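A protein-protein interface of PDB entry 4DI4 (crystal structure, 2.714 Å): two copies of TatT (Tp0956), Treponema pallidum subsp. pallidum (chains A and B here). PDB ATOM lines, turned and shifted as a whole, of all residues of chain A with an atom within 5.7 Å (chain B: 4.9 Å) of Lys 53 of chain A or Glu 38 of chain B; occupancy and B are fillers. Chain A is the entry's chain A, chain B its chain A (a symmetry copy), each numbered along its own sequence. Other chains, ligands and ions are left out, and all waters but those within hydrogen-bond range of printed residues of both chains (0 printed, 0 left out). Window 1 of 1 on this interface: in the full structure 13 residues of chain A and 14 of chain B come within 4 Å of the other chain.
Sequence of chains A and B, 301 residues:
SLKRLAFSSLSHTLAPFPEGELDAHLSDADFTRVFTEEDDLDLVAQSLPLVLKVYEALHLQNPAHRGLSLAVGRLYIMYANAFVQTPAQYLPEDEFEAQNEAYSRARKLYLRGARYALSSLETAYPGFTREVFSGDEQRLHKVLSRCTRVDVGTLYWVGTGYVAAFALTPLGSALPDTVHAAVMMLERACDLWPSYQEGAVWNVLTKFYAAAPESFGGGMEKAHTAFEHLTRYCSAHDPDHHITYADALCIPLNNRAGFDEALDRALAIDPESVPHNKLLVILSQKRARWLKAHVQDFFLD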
ATOM      1  N   LEU A  48      20.381 -17.090  11.406  1.00  0.00           N
ATOM      2  CA  LEU A  48      19.652 -15.928  10.865  1.00  0.00           C
ATOM      3  C   LEU A  48      18.761 -16.111   9.634  1.00  0.00           C
ATOM      4  O   LEU A  48      17.731 -15.456   9.523  1.00  0.00           O
ATOM      5  CB  LEU A  48      20.614 -14.790  10.552  1.00  0.00           C
ATOM      6  CG  LEU A  48      20.947 -13.869  11.704  1.00  0.00           C
ATOM      7  CD1 LEU A  48      21.596 -12.606  11.155  1.00  0.00           C
ATOM      8  CD2 LEU A  48      19.672 -13.574  12.429  1.00  0.00           C
ATOM      9  N   PRO A  49      19.182 -16.936   8.667  1.00  0.00           N
ATOM     10  CA  PRO A  49      18.362 -16.919   7.450  1.00  0.00           C
ATOM     11  C   PRO A  49      16.880 -17.163   7.725  1.00  0.00           C
ATOM     12  O   PRO A  49      16.066 -16.390   7.228  1.00  0.00           O
ATOM     13  CB  PRO A  49      18.967 -18.041   6.594  1.00  0.00           C
ATOM     14  CG  PRO A  49      20.388 -18.086   7.024  1.00  0.00           C
ATOM     15  CD  PRO A  49      20.393 -17.756   8.503  1.00  0.00           C
ATOM     16  N   LEU A  50      16.553 -18.173   8.528  1.00  0.00           N
ATOM     17  CA  LEU A  50      15.164 -18.467   8.883  1.00  0.00           C
ATOM     18  C   LEU A  50      14.473 -17.305   9.597  1.00  0.00           C
ATOM     19  O   LEU A  50      13.298 -17.020   9.340  1.00  0.00           O
ATOM     20  CB  LEU A  50      15.071 -19.741   9.725  1.00  0.00           C
ATOM     21  CG  LEU A  50      13.683 -20.343   9.973  1.00  0.00           C
ATOM     22  CD1 LEU A  50      12.852 -20.440   8.692  1.00  0.00           C
ATOM     23  CD2 LEU A  50      13.804 -21.713  10.656  1.00  0.00           C
ATOM     24  N   VAL A  51      15.208 -16.643  10.486  1.00  0.00           N
ATOM     25  CA  VAL A  51      14.690 -15.472  11.179  1.00  0.00           C
ATOM     26  C   VAL A  51      14.267 -14.375  10.212  1.00  0.00           C
ATOM     27  O   VAL A  51      13.243 -13.730  10.431  1.00  0.00           O
ATOM     28  CB  VAL A  51      15.701 -14.911  12.188  1.00  0.00           C
ATOM     29  CG1 VAL A  51      15.123 -13.703  12.905  1.00  0.00           C
ATOM     30  CG2 VAL A  51      16.056 -15.965  13.186  1.00  0.00           C
ATOM     31  N   LEU A  52      15.042 -14.153   9.152  1.00  0.00           N
ATOM     32  CA  LEU A  52      14.640 -13.170   8.143  1.00  0.00           C
ATOM     33  C   LEU A  52      13.404 -13.660   7.412  1.00  0.00           C
ATOM     34  O   LEU A  52      12.524 -12.872   7.092  1.00  0.00           O
ATOM     35  CB  LEU A  52      15.738 -12.912   7.102  1.00  0.00           C
ATOM     36  CG  LEU A  52      17.135 -12.494   7.521  1.00  0.00           C
ATOM     37  CD1 LEU A  52      18.081 -12.710   6.372  1.00  0.00           C
ATOM     38  CD2 LEU A  52      17.174 -11.079   7.945  1.00  0.00           C
ATOM     39  N   LYS A  53      13.352 -14.963   7.141  1.00  0.00           N
ATOM     40  CA  LYS A  53      12.281 -15.532   6.348  1.00  0.00           C
ATOM     41  C   LYS A  53      10.967 -15.341   7.070  1.00  0.00           C
ATOM     42  O   LYS A  53       9.942 -15.047   6.452  1.00  0.00           O
ATOM     43  CB  LYS A  53      12.515 -17.016   6.087  1.00  0.00           C
ATOM     44  CG  LYS A  53      13.664 -17.308   5.157  1.00  0.00           C
ATOM     45  CD  LYS A  53      13.286 -17.117   3.718  1.00  0.00           C
ATOM     46  CE  LYS A  53      13.105 -15.671   3.363  1.00  0.00           C
ATOM     47  NZ  LYS A  53      12.652 -15.528   1.950  1.00  0.00           N
ATOM     48  N   VAL A  54      11.024 -15.507   8.387  1.00  0.00           N
ATOM     49  CA  VAL A  54       9.873 -15.311   9.247  1.00  0.00           C
ATOM     50  C   VAL A  54       9.447 -13.855   9.293  1.00  0.00           C
ATOM     51  O   VAL A  54       8.277 -13.533   9.037  1.00  0.00           O
ATOM     52  CB  VAL A  54      10.146 -15.790  10.676  1.00  0.00           C
ATOM     53  CG1 VAL A  54       9.123 -15.207  11.623  1.00  0.00           C
ATOM     54  CG2 VAL A  54      10.112 -17.305  10.742  1.00  0.00           C
ATOM     55  N   TYR A  55      10.391 -12.977   9.626  1.00  0.00           N
ATOM     56  CA  TYR A  55      10.085 -11.552   9.705  1.00  0.00           C
ATOM     57  C   TYR A  55       9.515 -11.064   8.375  1.00  0.00           C
ATOM     58  O   TYR A  55       8.774 -10.087   8.317  1.00  0.00           O
ATOM     59  CB  TYR A  55      11.330 -10.748  10.052  1.00  0.00           C
ATOM     60  CG  TYR A  55      11.605 -10.550  11.518  1.00  0.00           C
ATOM     61  CD1 TYR A  55      11.882 -11.616  12.352  1.00  0.00           C
ATOM     62  CD2 TYR A  55      11.625  -9.275  12.061  1.00  0.00           C
ATOM     63  CE1 TYR A  55      12.149 -11.417  13.705  1.00  0.00           C
ATOM     64  CE2 TYR A  55      11.892  -9.063  13.404  1.00  0.00           C
ATOM     65  CZ  TYR A  55      12.153 -10.133  14.223  1.00  0.00           C
ATOM     66  OH  TYR A  55      12.416  -9.899  15.557  1.00  0.00           O
ATOM     67  N   GLU A  56       9.888 -11.743   7.298  1.00  0.00           N
ATOM     68  CA  GLU A  56       9.492 -11.311   5.973  1.00  0.00           C
ATOM     69  C   GLU A  56       8.062 -11.763   5.721  1.00  0.00           C
ATOM     70  O   GLU A  56       7.229 -11.010   5.217  1.00  0.00           O
ATOM     71  CB  GLU A  56      10.418 -11.931   4.950  1.00  0.00           C
ATOM     72  CG  GLU A  56      10.769 -11.057   3.774  1.00  0.00           C
ATOM     73  CD  GLU A  56      11.688 -11.789   2.805  1.00  0.00           C
ATOM     74  OE1 GLU A  56      12.157 -12.897   3.145  1.00  0.00           O
ATOM     75  OE2 GLU A  56      11.941 -11.266   1.706  1.00  0.00           O
ATOM     76  N   ALA A  57       7.791 -13.005   6.097  1.00  0.00           N
ATOM     77  CA  ALA A  57       6.468 -13.582   5.958  1.00  0.00           C
ATOM     78  C   ALA A  57       5.471 -12.757   6.791  1.00  0.00           C
ATOM     79  O   ALA A  57       4.398 -12.372   6.318  1.00  0.00           O
ATOM     80  CB  ALA A  57       6.491 -15.046   6.390  1.00  0.00           C
ATOM     81  N   LEU A  58       5.854 -12.462   8.023  1.00  0.00           N
ATOM     82  CA  LEU A  58       5.112 -11.524   8.835  1.00  0.00           C
ATOM     83  C   LEU A  58       4.840 -10.219   8.112  1.00  0.00           C
ATOM     84  O   LEU A  58       3.703  -9.757   8.040  1.00  0.00           O
ATOM     85  CB  LEU A  58       5.881 -11.229  10.110  1.00  0.00           C
ATOM     86  CG  LEU A  58       5.782 -12.416  11.044  1.00  0.00           C
ATOM     87  CD1 LEU A  58       6.312 -12.053  12.406  1.00  0.00           C
ATOM     88  CD2 LEU A  58       4.331 -12.804  11.118  1.00  0.00           C
ATOM     89  N   TYR A  76      17.930  -7.703   6.619  1.00  0.00           N
ATOM     90  CA  TYR A  76      18.473  -8.002   5.315  1.00  0.00           C
ATOM     91  C   TYR A  76      19.776  -7.246   5.037  1.00  0.00           C
ATOM     92  O   TYR A  76      20.776  -7.828   4.629  1.00  0.00           O
ATOM     93  CB  TYR A  76      17.414  -7.767   4.234  1.00  0.00           C
ATOM     94  CG  TYR A  76      16.750  -9.064   3.937  1.00  0.00           C
ATOM     95  CD1 TYR A  76      15.529  -9.381   4.493  1.00  0.00           C
ATOM     96  CD2 TYR A  76      17.397 -10.029   3.182  1.00  0.00           C
ATOM     97  CE1 TYR A  76      14.933 -10.601   4.261  1.00  0.00           C
ATOM     98  CE2 TYR A  76      16.810 -11.250   2.937  1.00  0.00           C
ATOM     99  CZ  TYR A  76      15.576 -11.530   3.481  1.00  0.00           C
ATOM    100  OH  TYR A  76      14.988 -12.741   3.243  1.00  0.00           O
ATOM    101  N   ARG A 112      16.931  -5.253  -1.429  1.00  0.00           N
ATOM    102  CA  ARG A 112      15.683  -5.838  -1.005  1.00  0.00           C
ATOM    103  C   ARG A 112      15.379  -5.285   0.367  1.00  0.00           C
ATOM    104  O   ARG A 112      14.243  -4.915   0.652  1.00  0.00           O
ATOM    105  CB  ARG A 112      15.816  -7.351  -0.924  1.00  0.00           C
ATOM    106  CG  ARG A 112      14.540  -8.078  -0.613  1.00  0.00           C
ATOM    107  CD  ARG A 112      14.821  -9.490  -0.109  1.00  0.00           C
ATOM    108  NE  ARG A 112      15.249 -10.399  -1.175  1.00  0.00           N
ATOM    109  CZ  ARG A 112      15.267 -11.725  -1.055  1.00  0.00           C
ATOM    110  NH1 ARG A 112      14.866 -12.303   0.075  1.00  0.00           N
ATOM    111  NH2 ARG A 112      15.673 -12.477  -2.071  1.00  0.00           N
ATOM    112  N   ARG B  33       5.091 -18.489   0.525  1.00  0.00           N
ATOM    113  CA  ARG B  33       5.426 -17.475  -0.466  1.00  0.00           C
ATOM    114  C   ARG B  33       6.870 -16.948  -0.352  1.00  0.00           C
ATOM    115  O   ARG B  33       7.565 -16.815  -1.368  1.00  0.00           O
ATOM    116  CB  ARG B  33       4.443 -16.315  -0.389  1.00  0.00           C
ATOM    117  CG  ARG B  33       3.409 -16.303  -1.475  1.00  0.00           C
ATOM    118  CD  ARG B  33       2.545 -15.020  -1.366  1.00  0.00           C
ATOM    119  NE  ARG B  33       3.295 -13.828  -1.734  1.00  0.00           N
ATOM    120  CZ  ARG B  33       2.979 -12.593  -1.338  1.00  0.00           C
ATOM    121  NH1 ARG B  33       1.938 -12.388  -0.512  1.00  0.00           N
ATOM    122  NH2 ARG B  33       3.713 -11.552  -1.754  1.00  0.00           N
ATOM    123  N   VAL B  34       7.316 -16.647   0.870  1.00  0.00           N
ATOM    124  CA  VAL B  34       8.681 -16.190   1.086  1.00  0.00           C
ATOM    125  C   VAL B  34       9.723 -17.211   0.640  1.00  0.00           C
ATOM    126  O   VAL B  34      10.899 -16.876   0.480  1.00  0.00           O
ATOM    127  CB  VAL B  34       8.986 -15.801   2.554  1.00  0.00           C
ATOM    128  CG1 VAL B  34       8.205 -14.570   2.976  1.00  0.00           C
ATOM    129  CG2 VAL B  34       8.758 -16.969   3.504  1.00  0.00           C
ATOM    130  N   PHE B  35       9.308 -18.458   0.470  1.00  0.00           N
ATOM    131  CA  PHE B  35      10.207 -19.485  -0.069  1.00  0.00           C
ATOM    132  C   PHE B  35      10.092 -19.642  -1.589  1.00  0.00           C
ATOM    133  O   PHE B  35      11.096 -19.541  -2.297  1.00  0.00           O
ATOM    134  CB  PHE B  35      10.060 -20.823   0.655  1.00  0.00           C
ATOM    135  CG  PHE B  35      10.502 -20.783   2.089  1.00  0.00           C
ATOM    136  CD1 PHE B  35      11.843 -20.853   2.415  1.00  0.00           C
ATOM    137  CD2 PHE B  35       9.574 -20.691   3.116  1.00  0.00           C
ATOM    138  CE1 PHE B  35      12.253 -20.818   3.734  1.00  0.00           C
ATOM    139  CE2 PHE B  35       9.976 -20.661   4.446  1.00  0.00           C
ATOM    140  CZ  PHE B  35      11.312 -20.718   4.754  1.00  0.00           C
ATOM    141  N   THR B  36       8.887 -19.949  -2.072  1.00  0.00           N
ATOM    142  CA  THR B  36       8.678 -20.212  -3.496  1.00  0.00           C
ATOM    143  C   THR B  36       8.938 -19.022  -4.417  1.00  0.00           C
ATOM    144  O   THR B  36       9.268 -19.199  -5.586  1.00  0.00           O
ATOM    145  CB  THR B  36       7.257 -20.708  -3.791  1.00  0.00           C
ATOM    146  OG1 THR B  36       6.326 -19.661  -3.502  1.00  0.00           O
ATOM    147  CG2 THR B  36       6.941 -21.934  -2.969  1.00  0.00           C
ATOM    148  N   GLU B  37       8.735 -17.822  -3.907  1.00  0.00           N
ATOM    149  CA  GLU B  37       8.925 -16.617  -4.707  1.00  0.00           C
ATOM    150  C   GLU B  37      10.282 -15.954  -4.478  1.00  0.00           C
ATOM    151  O   GLU B  37      10.552 -14.845  -4.964  1.00  0.00           O
ATOM    152  CB  GLU B  37       7.755 -15.664  -4.502  1.00  0.00           C
ATOM    153  CG  GLU B  37       6.431 -16.369  -4.713  1.00  0.00           C
ATOM    154  CD  GLU B  37       6.372 -17.112  -6.041  1.00  0.00           C
ATOM    155  OE1 GLU B  37       6.411 -16.458  -7.115  1.00  0.00           O
ATOM    156  OE2 GLU B  37       6.286 -18.357  -6.007  1.00  0.00           O
ATOM    157  N   GLU B  38      11.106 -16.648  -3.697  1.00  0.00           N
ATOM    158  CA  GLU B  38      12.478 -16.262  -3.386  1.00  0.00           C
ATOM    159  C   GLU B  38      13.409 -16.400  -4.612  1.00  0.00           C
ATOM    160  O   GLU B  38      13.227 -17.295  -5.438  1.00  0.00           O
ATOM    161  CB  GLU B  38      12.971 -17.149  -2.236  1.00  0.00           C
ATOM    162  CG  GLU B  38      14.393 -16.962  -1.819  1.00  0.00           C
ATOM    163  CD  GLU B  38      14.668 -15.598  -1.214  1.00  0.00           C
ATOM    164  OE1 GLU B  38      14.432 -15.427   0.006  1.00  0.00           O
ATOM    165  OE2 GLU B  38      15.144 -14.704  -1.962  1.00  0.00           O
ATOM    166  N   ASP B  39      14.340 -15.460  -4.771  1.00  0.00           N
ATOM    167  CA  ASP B  39      15.423 -15.572  -5.755  1.00  0.00           C
ATOM    168  C   ASP B  39      16.810 -15.967  -5.205  1.00  0.00           C
ATOM    169  O   ASP B  39      17.759 -16.091  -5.967  1.00  0.00           O
ATOM    170  CB  ASP B  39      15.555 -14.285  -6.575  1.00  0.00           C
ATOM    171  CG  ASP B  39      15.938 -13.098  -5.725  1.00  0.00           C
ATOM    172  OD1 ASP B  39      17.049 -13.078  -5.157  1.00  0.00           O
ATOM    173  OD2 ASP B  39      15.125 -12.170  -5.626  1.00  0.00           O
ATOM    174  N   ASP B  40      16.951 -16.136  -3.897  1.00  0.00           N
ATOM    175  CA  ASP B  40      18.264 -16.428  -3.331  1.00  0.00           C
ATOM    176  C   ASP B  40      18.340 -17.885  -2.884  1.00  0.00           C
ATOM    177  O   ASP B  40      17.725 -18.264  -1.884  1.00  0.00           O
ATOM    178  CB  ASP B  40      18.539 -15.507  -2.145  1.00  0.00           C
ATOM    179  CG  ASP B  40      20.002 -15.491  -1.737  1.00  0.00           C
ATOM    180  OD1 ASP B  40      20.479 -16.498  -1.178  1.00  0.00           O
ATOM    181  OD2 ASP B  40      20.668 -14.457  -1.964  1.00  0.00           O
ATOM    182  N   LEU B  43      19.936 -18.624   0.799  1.00  0.00           N
ATOM    183  CA  LEU B  43      18.966 -18.302   1.829  1.00  0.00           C
ATOM    184  C   LEU B  43      17.955 -19.422   2.000  1.00  0.00           C
ATOM    185  O   LEU B  43      17.784 -19.940   3.112  1.00  0.00           O
ATOM    186  CB  LEU B  43      18.243 -17.013   1.496  1.00  0.00           C
ATOM    187  CG  LEU B  43      18.900 -15.778   2.088  1.00  0.00           C
ATOM    188  CD1 LEU B  43      18.212 -14.506   1.609  1.00  0.00           C
ATOM    189  CD2 LEU B  43      18.868 -15.906   3.594  1.00  0.00           C
ATOM    190  N   VAL B  44      17.296 -19.820   0.914  1.00  0.00           N
ATOM    191  CA  VAL B  44      16.329 -20.904   1.043  1.00  0.00           C
ATOM    192  C   VAL B  44      16.981 -22.136   1.668  1.00  0.00           C
ATOM    193  O   VAL B  44      16.432 -22.740   2.581  1.00  0.00           O
ATOM    194  CB  VAL B  44      15.636 -21.241  -0.279  1.00  0.00           C
ATOM    195  CG1 VAL B  44      14.795 -22.516  -0.134  1.00  0.00           C
ATOM    196  CG2 VAL B  44      14.764 -20.094  -0.704  1.00  0.00           C
ATOM    197  N   SER B  47      17.637 -21.836   5.484  1.00  0.00           N
ATOM    198  CA  SER B  47      16.439 -21.795   6.304  1.00  0.00           C
ATOM    199  C   SER B  47      15.581 -23.078   6.351  1.00  0.00           C
ATOM    200  O   SER B  47      14.998 -23.384   7.390  1.00  0.00           O
ATOM    201  CB  SER B  47      15.598 -20.558   5.987  1.00  0.00           C
ATOM    202  OG  SER B  47      15.219 -20.510   4.630  1.00  0.00           O
ATOM    203  N   LYS B 278       8.795 -18.386  -8.656  1.00  0.00           N
ATOM    204  CA  LYS B 278      10.024 -17.741  -9.117  1.00  0.00           C
ATOM    205  C   LYS B 278      11.296 -18.565  -8.806  1.00  0.00           C
ATOM    206  O   LYS B 278      12.130 -18.779  -9.688  1.00  0.00           O
ATOM    207  CB  LYS B 278      10.154 -16.325  -8.543  1.00  0.00           C
ATOM    208  CG  LYS B 278      11.083 -15.434  -9.353  1.00  0.00           C
ATOM    209  CD  LYS B 278      10.999 -13.973  -8.956  1.00  0.00           C
ATOM    210  CE  LYS B 278      11.843 -13.681  -7.729  1.00  0.00           C
ATOM    211  NZ  LYS B 278      11.756 -12.248  -7.302  1.00  0.00           N
ATOM    212  N   LEU B 279      11.429 -19.022  -7.560  1.00  0.00           N
ATOM    213  CA  LEU B 279      12.529 -19.876  -7.138  1.00  0.00           C
ATOM    214  C   LEU B 279      12.773 -21.059  -8.064  1.00  0.00           C
ATOM    215  O   LEU B 279      13.907 -21.352  -8.416  1.00  0.00           O
ATOM    216  CB  LEU B 279      12.291 -20.432  -5.730  1.00  0.00           C
ATOM    217  CG  LEU B 279      13.556 -21.139  -5.213  1.00  0.00           C
ATOM    218  CD1 LEU B 279      14.555 -20.132  -4.686  1.00  0.00           C
ATOM    219  CD2 LEU B 279      13.277 -22.166  -4.153  1.00  0.00           C
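Pro 49 of chain A touches Leu 43 of chain B (CB to CD2, 3.7 Å).
Leu 50 of chain A touches Ser 47 of chain B.
Phe 35 of chain B touches Lys 53 of chain A (CE1 to CD, 3.8 Å).
Ser 47 of chain B touches Lys 53 of chain A (OG to CG, 3.6 Å).
C of Glu 56 of chain A touches CG1 of Val 34 of chain B, 3.9 Å away.
CG1 of Val 34 of chain B touches N of Ala 57 of chain A (3.5 Å).
CD1 of Leu 43 of chain B touches CE2 of Tyr 76 of chain A, at 3.8 Å.
The side-chain amino group of Lys 53 of chain A lies within salt-bridge range of the side-chain carboxylate of Glu 38 of chain B (2.6 Å).
The side-chain carboxylate of Asp 39 of chain B is in salt-bridge range of the guanidinium group of Arg 112 of chain A (3.4 Å).
The side-chain carboxylate (OE1) of Glu 38 of chain B lies within salt-bridge range of the guanidinium group (NH1) of Arg 112 of chain A (3.2 Å).
O of Val 34 of chain B is in hydrogen-bond range of NZ of Lys 53 of chain A, 2.7 Å away.
OD1 of Asp 40 of chain B is in hydrogen-bond range of N of Leu 43 of chain B, at 3.0 Å.
The backbone NH (N) of Leu 279 of chain B lies close to the backbone carbonyl oxygen (O) of Glu 38 of chain B (3.3 Å).
The side-chain carboxylate of Glu 38 of chain B sits at hydrogen-bond distance from the backbone NH of Asp 40 of chain B (3.0 Å).
The side-chain carboxylate of Glu 56 of chain A is in salt-bridge range of the side-chain amino group of Lys 53 of chain A.
O of Val 44 of chain B lies within hydrogen-bond range of OG of Ser 47 of chain B, at 3.3 Å.
The backbone carbonyl oxygen (O) of Leu 43 of chain B lies within hydrogen-bond range of the side-chain hydroxyl (OG) of Ser 47 of chain B.
No position is printed for both chains.
Lys 53 of chain A touches four residues of chain B.
Printed residues of chain A within 4 Å of Ser 47 of chain B: Leu 50 and Lys 53.
Printed residues of chain A within 4 Å of Val 34 of chain B: Lys 53 (2.7 Å), Glu 56 (3.9 Å) and Ala 57 (3.5 Å).
Of the printed residues of chain A, Asp 39 of chain B touches Arg 112.
Glu 37 of chain B touches none of the printed residues of chain A.
Hydrophobic or aromatic side chains of chain A within 4 Å of the printed part of chain B: Pro 49, Leu 50, Ala 57 and Tyr 76.
Hydrophobic or aromatic side chains of chain B within 4 Å of the printed part of chain A: Val 34, Phe 35 and Leu 43.
Among the printed residues, 11 pairs touch across the chains.
Among the printed residues, Asp or Glu carboxylates within 4 Å of a Lys or Arg side-chain nitrogen of the other chain: Lys 53 of chain A with Glu 38 of chain B (2.6 Å), Arg 112 of chain A with Glu 38 of chain B (2.3 Å) and Arg 112 of chain A with Asp 39 of chain B (3.4 Å).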
